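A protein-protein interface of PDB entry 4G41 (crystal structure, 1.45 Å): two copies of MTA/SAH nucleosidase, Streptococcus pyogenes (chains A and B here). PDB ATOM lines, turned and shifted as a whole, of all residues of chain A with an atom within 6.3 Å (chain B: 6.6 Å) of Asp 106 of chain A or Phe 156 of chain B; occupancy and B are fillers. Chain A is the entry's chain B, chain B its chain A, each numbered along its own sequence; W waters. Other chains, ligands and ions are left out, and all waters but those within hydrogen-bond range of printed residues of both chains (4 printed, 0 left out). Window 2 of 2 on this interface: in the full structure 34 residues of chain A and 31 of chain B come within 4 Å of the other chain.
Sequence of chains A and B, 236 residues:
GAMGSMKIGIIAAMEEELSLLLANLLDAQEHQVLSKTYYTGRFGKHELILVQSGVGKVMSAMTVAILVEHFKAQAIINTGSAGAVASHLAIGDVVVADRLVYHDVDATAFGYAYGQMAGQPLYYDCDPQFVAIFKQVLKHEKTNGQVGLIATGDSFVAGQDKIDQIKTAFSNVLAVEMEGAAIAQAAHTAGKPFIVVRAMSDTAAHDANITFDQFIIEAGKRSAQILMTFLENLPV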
ATOM      1  N   ASP A 104      22.392  19.992 -27.186  1.00  0.00           N
ATOM      2  CA  ASP A 104      22.706  20.428 -25.825  1.00  0.00           C
ATOM      3  C   ASP A 104      22.911  19.249 -24.872  1.00  0.00           C
ATOM      4  O   ASP A 104      22.895  19.488 -23.678  1.00  0.00           O
ATOM      5  CB  ASP A 104      21.602  21.396 -25.305  1.00  0.00           C
ATOM      6  CG  ASP A 104      20.270  20.729 -25.042  1.00  0.00           C
ATOM      7  OD1 ASP A 104      20.086  19.566 -25.475  1.00  0.00           O
ATOM      8  OD2 ASP A 104      19.432  21.430 -24.389  1.00  0.00           O
ATOM      9  N   VAL A 105      23.059  18.007 -25.360  1.00  0.00           N
ATOM     10  CA  VAL A 105      23.248  16.850 -24.528  1.00  0.00           C
ATOM     11  C   VAL A 105      24.713  16.467 -24.507  1.00  0.00           C
ATOM     12  O   VAL A 105      25.329  16.238 -25.564  1.00  0.00           O
ATOM     13  CB  VAL A 105      22.360  15.710 -25.095  1.00  0.00           C
ATOM     14  CG1 VAL A 105      22.746  14.345 -24.473  1.00  0.00           C
ATOM     15  CG2 VAL A 105      20.879  16.026 -24.801  1.00  0.00           C
ATOM     16  N   ASP A 106      25.230  16.435 -23.267  1.00  0.00           N
ATOM     17  CA  ASP A 106      26.648  16.002 -23.108  1.00  0.00           C
ATOM     18  C   ASP A 106      26.702  14.930 -22.018  1.00  0.00           C
ATOM     19  O   ASP A 106      26.792  15.236 -20.819  1.00  0.00           O
ATOM     20  CB  ASP A 106      27.532  17.188 -22.761  1.00  0.00           C
ATOM     21  CG  ASP A 106      28.998  16.834 -22.717  1.00  0.00           C
ATOM     22  OD1 ASP A 106      29.328  15.638 -22.616  1.00  0.00           O
ATOM     23  OD2 ASP A 106      29.813  17.812 -22.837  1.00  0.00           O
ATOM     24  N   ALA A 107      26.680  13.663 -22.469  1.00  0.00           N
ATOM     25  CA  ALA A 107      26.978  12.493 -21.633  1.00  0.00           C
ATOM     26  C   ALA A 107      28.277  11.847 -22.100  1.00  0.00           C
ATOM     27  O   ALA A 107      28.464  10.609 -21.872  1.00  0.00           O
ATOM     28  CB  ALA A 107      25.787  11.547 -21.660  1.00  0.00           C
ATOM     29  N   THR A 108      29.185  12.671 -22.630  1.00  0.00           N
ATOM     30  CA  THR A 108      30.500  12.155 -23.107  1.00  0.00           C
ATOM     31  C   THR A 108      31.318  11.582 -21.949  1.00  0.00           C
ATOM     32  O   THR A 108      32.160  10.687 -22.184  1.00  0.00           O
ATOM     33  CB  THR A 108      31.326  13.217 -23.822  1.00  0.00           C
ATOM     34  OG1 THR A 108      31.619  14.293 -22.893  1.00  0.00           O
ATOM     35  CG2 THR A 108      30.572  13.755 -25.003  1.00  0.00           C
ATOM     36  N   ALA A 109      31.079  12.026 -20.732  1.00  0.00           N
ATOM     37  CA  ALA A 109      31.836  11.487 -19.566  1.00  0.00           C
ATOM     38  C   ALA A 109      31.552   9.970 -19.412  1.00  0.00           C
ATOM     39  O   ALA A 109      32.421   9.283 -18.824  1.00  0.00           O
ATOM     40  CB  ALA A 109      31.488  12.272 -18.295  1.00  0.00           C
ATOM     41  N   PHE A 110      30.383   9.490 -19.853  1.00  0.00           N
ATOM     42  CA  PHE A 110      30.031   8.056 -19.823  1.00  0.00           C
ATOM     43  C   PHE A 110      30.347   7.365 -21.154  1.00  0.00           C
ATOM     44  O   PHE A 110      29.947   6.164 -21.251  1.00  0.00           O
ATOM     45  CB  PHE A 110      28.606   7.851 -19.483  1.00  0.00           C
ATOM     46  N   TYR A 112      29.524   8.291 -24.298  1.00  0.00           N
ATOM     47  CA  TYR A 112      28.626   8.541 -25.435  1.00  0.00           C
ATOM     48  C   TYR A 112      29.104   9.620 -26.403  1.00  0.00           C
ATOM     49  O   TYR A 112      30.032  10.439 -26.042  1.00  0.00           O
ATOM     50  CB  TYR A 112      27.220   8.958 -24.876  1.00  0.00           C
ATOM     51  CG  TYR A 112      26.530   7.841 -24.162  1.00  0.00           C
ATOM     52  CD1 TYR A 112      25.959   6.805 -24.877  1.00  0.00           C
ATOM     53  CD2 TYR A 112      26.573   7.767 -22.722  1.00  0.00           C
ATOM     54  CE1 TYR A 112      25.334   5.750 -24.201  1.00  0.00           C
ATOM     55  CE2 TYR A 112      25.981   6.722 -22.066  1.00  0.00           C
ATOM     56  CZ  TYR A 112      25.364   5.760 -22.811  1.00  0.00           C
ATOM     57  OH  TYR A 112      24.818   4.647 -22.181  1.00  0.00           O
ATOM     58  N   ALA A 113      28.537   9.668 -27.625  1.00  0.00           N
ATOM     59  CA  ALA A 113      28.913  10.686 -28.565  1.00  0.00           C
ATOM     60  C   ALA A 113      28.361  12.031 -28.064  1.00  0.00           C
ATOM     61  O   ALA A 113      27.276  12.080 -27.390  1.00  0.00           O
ATOM     62  CB  ALA A 113      28.299  10.437 -29.914  1.00  0.00           C
ATOM     63  N   TYR A 114      29.017  13.164 -28.369  1.00  0.00           N
ATOM     64  CA  TYR A 114      28.403  14.425 -28.052  1.00  0.00           C
ATOM     65  C   TYR A 114      26.997  14.510 -28.735  1.00  0.00           C
ATOM     66  O   TYR A 114      26.847  14.241 -29.939  1.00  0.00           O
ATOM     67  CB  TYR A 114      29.320  15.659 -28.540  1.00  0.00           C
ATOM     68  CG  TYR A 114      28.635  16.936 -28.086  1.00  0.00           C
ATOM     69  CD1 TYR A 114      28.840  17.384 -26.797  1.00  0.00           C
ATOM     70  CD2 TYR A 114      27.683  17.593 -28.908  1.00  0.00           C
ATOM     71  CE1 TYR A 114      28.117  18.509 -26.339  1.00  0.00           C
ATOM     72  CE2 TYR A 114      26.956  18.726 -28.462  1.00  0.00           C
ATOM     73  CZ  TYR A 114      27.154  19.099 -27.152  1.00  0.00           C
ATOM     74  OH  TYR A 114      26.501  20.204 -26.550  1.00  0.00           O
ATOM     75  N   GLY A 115      25.991  14.946 -27.935  1.00  0.00           N
ATOM     76  CA  GLY A 115      24.612  15.026 -28.437  1.00  0.00           C
ATOM     77  C   GLY A 115      23.805  13.803 -28.131  1.00  0.00           C
ATOM     78  O   GLY A 115      22.573  13.910 -28.221  1.00  0.00           O
ATOM     79  N   GLN A 116      24.428  12.664 -27.791  1.00  0.00           N
ATOM     80  CA  GLN A 116      23.689  11.383 -27.651  1.00  0.00           C
ATOM     81  C   GLN A 116      23.234  11.195 -26.237  1.00  0.00           C
ATOM     82  O   GLN A 116      24.019  11.190 -25.299  1.00  0.00           O
ATOM     83  CB  GLN A 116      24.646  10.253 -28.037  1.00  0.00           C
ATOM     84  CG  GLN A 116      24.020   8.882 -27.877  1.00  0.00           C
ATOM     85  CD  GLN A 116      25.008   7.762 -28.170  1.00  0.00           C
ATOM     86  OE1 GLN A 116      26.218   7.975 -28.241  1.00  0.00           O
ATOM     87  NE2 GLN A 116      24.497   6.565 -28.330  1.00  0.00           N
ATOM     88  N   GLY B 153      19.989  18.969 -15.583  1.00  0.00           N
ATOM     89  CA  GLY B 153      20.137  19.249 -16.961  1.00  0.00           C
ATOM     90  C   GLY B 153      20.333  17.954 -17.707  1.00  0.00           C
ATOM     91  O   GLY B 153      20.672  16.914 -17.078  1.00  0.00           O
ATOM     92  N   ASP B 154      20.207  17.997 -19.035  1.00  0.00           N
ATOM     93  CA  ASP B 154      20.323  16.810 -19.912  1.00  0.00           C
ATOM     94  C   ASP B 154      21.790  16.539 -20.281  1.00  0.00           C
ATOM     95  O   ASP B 154      22.130  16.120 -21.381  1.00  0.00           O
ATOM     96  CB  ASP B 154      19.499  17.030 -21.194  1.00  0.00           C
ATOM     97  CG  ASP B 154      18.277  16.098 -21.318  1.00  0.00           C
ATOM     98  OD1 ASP B 154      18.041  15.372 -20.371  1.00  0.00           O
ATOM     99  OD2 ASP B 154      17.702  16.183 -22.443  1.00  0.00           O
ATOM    100  N   SER B 155      22.665  16.718 -19.300  1.00  0.00           N
ATOM    101  CA  SER B 155      24.126  16.441 -19.444  1.00  0.00           C
ATOM    102  C   SER B 155      24.610  15.871 -18.168  1.00  0.00           C
ATOM    103  O   SER B 155      24.104  16.242 -17.075  1.00  0.00           O
ATOM    104  CB  SER B 155      24.897  17.725 -19.742  1.00  0.00           C
ATOM    105  OG  SER B 155      24.544  18.208 -21.018  1.00  0.00           O
ATOM    106  N   PHE B 156      25.641  14.999 -18.231  1.00  0.00           N
ATOM    107  CA  PHE B 156      26.397  14.653 -17.030  1.00  0.00           C
ATOM    108  C   PHE B 156      27.586  15.648 -16.944  1.00  0.00           C
ATOM    109  O   PHE B 156      28.441  15.691 -17.828  1.00  0.00           O
ATOM    110  CB  PHE B 156      26.976  13.260 -17.061  1.00  0.00           C
ATOM    111  CG  PHE B 156      27.663  12.954 -15.779  1.00  0.00           C
ATOM    112  CD1 PHE B 156      26.914  12.519 -14.718  1.00  0.00           C
ATOM    113  CD2 PHE B 156      29.043  13.202 -15.601  1.00  0.00           C
ATOM    114  CE1 PHE B 156      27.517  12.238 -13.504  1.00  0.00           C
ATOM    115  CE2 PHE B 156      29.623  12.931 -14.329  1.00  0.00           C
ATOM    116  CZ  PHE B 156      28.833  12.464 -13.324  1.00  0.00           C
ATOM    117  N   VAL B 157      27.564  16.470 -15.917  1.00  0.00           N
ATOM    118  CA  VAL B 157      28.563  17.582 -15.802  1.00  0.00           C
ATOM    119  C   VAL B 157      29.703  17.122 -14.915  1.00  0.00           C
ATOM    120  O   VAL B 157      29.571  16.939 -13.703  1.00  0.00           O
ATOM    121  CB  VAL B 157      27.871  18.832 -15.197  1.00  0.00           C
ATOM    122  CG1 VAL B 157      28.924  19.945 -15.168  1.00  0.00           C
ATOM    123  CG2 VAL B 157      26.700  19.250 -16.057  1.00  0.00           C
ATOM    124  N   ALA B 158      30.798  16.796 -15.622  1.00  0.00           N
ATOM    125  CA  ALA B 158      31.979  16.192 -14.996  1.00  0.00           C
ATOM    126  C   ALA B 158      33.012  17.265 -14.740  1.00  0.00           C
ATOM    127  O   ALA B 158      33.814  17.091 -13.818  1.00  0.00           O
ATOM    128  CB  ALA B 158      32.536  15.120 -15.939  1.00  0.00           C
ATOM    129  N   GLY B 159      33.067  18.325 -15.537  1.00  0.00           N
ATOM    130  CA  GLY B 159      34.146  19.312 -15.318  1.00  0.00           C
ATOM    131  C   GLY B 159      33.851  20.230 -14.145  1.00  0.00           C
ATOM    132  O   GLY B 159      32.738  20.771 -14.052  1.00  0.00           O
ATOM    133  N   LYS B 162      32.580  23.742 -15.005  1.00  0.00           N
ATOM    134  CA  LYS B 162      31.148  23.827 -15.284  1.00  0.00           C
ATOM    135  C   LYS B 162      30.310  23.711 -13.997  1.00  0.00           C
ATOM    136  O   LYS B 162      29.264  24.405 -13.912  1.00  0.00           O
ATOM    137  CB  LYS B 162      30.735  22.801 -16.304  1.00  0.00           C
ATOM    138  CG  LYS B 162      31.343  23.075 -17.687  1.00  0.00           C
ATOM    139  CD  LYS B 162      31.387  21.733 -18.450  1.00  0.00           C
ATOM    140  CE  LYS B 162      31.043  21.757 -19.954  1.00  0.00           C
ATOM    141  NZ  LYS B 162      32.209  21.398 -20.832  1.00  0.00           N
ATOM    142  N   VAL B 176      23.545  18.252  -8.406  1.00  0.00           N
ATOM    143  CA  VAL B 176      23.218  18.455  -9.825  1.00  0.00           C
ATOM    144  C   VAL B 176      23.016  17.063 -10.444  1.00  0.00           C
ATOM    145  O   VAL B 176      23.817  16.123 -10.165  1.00  0.00           O
ATOM    146  CB  VAL B 176      24.400  19.182 -10.542  1.00  0.00           C
ATOM    147  CG1 VAL B 176      24.222  19.184 -12.035  1.00  0.00           C
ATOM    148  CG2 VAL B 176      24.557  20.629 -10.098  1.00  0.00           C
ATOM    149  N   MET B 178      20.247  14.642 -13.567  1.00  0.00           N
ATOM    150  CA  MET B 178      19.728  14.622 -14.949  1.00  0.00           C
ATOM    151  C   MET B 178      18.217  14.412 -15.030  1.00  0.00           C
ATOM    152  O   MET B 178      17.682  14.401 -16.182  1.00  0.00           O
ATOM    153  CB  MET B 178      20.460  13.568 -15.786  1.00  0.00           C
ATOM    154  CG  MET B 178      21.931  14.000 -15.952  1.00  0.00           C
ATOM    155  SD  MET B 178      22.784  12.753 -16.979  1.00  0.00           S
ATOM    156  CE  MET B 178      22.103  13.085 -18.574  1.00  0.00           C
HETATM  157  O   HOH W   1      29.605  14.498 -19.944  1.00  0.00           O
HETATM  158  O   HOH W   2      28.660  18.258 -19.584  1.00  0.00           O
HETATM  159  O   HOH W   3      22.456  19.963 -21.076  1.00  0.00           O
HETATM  160  O   HOH W   4      25.825  20.481 -22.506  1.00  0.00           O
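No position is printed for both chains. Of the 8 pairs that touch across the chains among the printed residues, none has its exchanged pair printed and touching as well.
Of the 10 printed residues of chain B, 4 touch a printed residue of chain A. Of the 12 printed residues of chain A, 4 touch a printed residue of chain B. Among the printed residues, 8 pairs touch across the chains.
The backbone NH of Asp 106 of chain A is in hydrogen-bond range of the side-chain hydroxyl of Ser 155 of chain B, 2.9 Å away. O of Asp 104 of chain A sits at hydrogen-bond distance from OG of Ser 155 of chain B, at 3.4 Å. The backbone NH (N) of Phe 156 of chain B lies within hydrogen-bond range of the backbone carbonyl oxygen (O) of Asp 106 of chain A.
Water W3 bridges the backbone carbonyl oxygen (O) of Asp 104 of chain A (2.7 Å) and the side-chain hydroxyl (OG) of Ser 155 of chain B (2.7 Å). Water W1 lies within hydrogen-bond range of O of Phe 156 of chain B, OD1 of Asp 106 of chain A, N of Ala 109 of chain A and N of Thr 108 of chain A. Water W4 lies within hydrogen-bond range of OG of Ser 155 of chain B (3.0 Å) and O of Asp 104 of chain A (3.3 Å). Water W2 lies within hydrogen-bond range of O of Phe 156 of chain B (3.1 Å) and OD2 of Asp 106 of chain A (3.5 Å).
Among the printed residues, merely in contact across the chains: Val 105 of chain A with Asp 154 of chain B, Asp 106 of chain A with Asp 154 of chain B, Ala 109 of chain A with Phe 156 of chain B, Ala 109 of chain A with Ala 158 of chain B and Val 105 of chain A with Ser 155 of chain B.
The side-chain hydroxyl of Thr 108 of chain A is in hydrogen-bond range of the side-chain carboxylate of Asp 106 of chain A. N of Gly 115 of chain A lies within hydrogen-bond range of O of Val 105 of chain A (2.8 Å).
Printed residues of chain B within 4 Å of Asp 104 of chain A: Ser 155. Printed residues of chain B within 4 Å of Val 105 of chain A: Asp 154 and Ser 155. Asp 106 of chain A touches just these residues of chain B: Asp 154, Ser 155 and Phe 156. Gly 153 of chain B touches none of the printed residues of chain A. Printed residues of chain A within 4 Å of Ser 155 of chain B: Asp 104, Val 105 and Asp 106. Phe 156 of chain B touches just these residues of chain A: Asp 106 and Ala 109. Lys 162 of chain B touches none of the printed residues of chain A. The nearest residue of chain B that does not touch Asp 106 of chain A is Lys 162 of chain B (4.8 Å). The nearest residue of chain A that does not touch Phe 156 of chain B is Ala 107 of chain A (4.4 Å). The nearest printed residue of chain B that does not touch Val 105 of chain A is Met 178 of chain B (6.1 Å).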
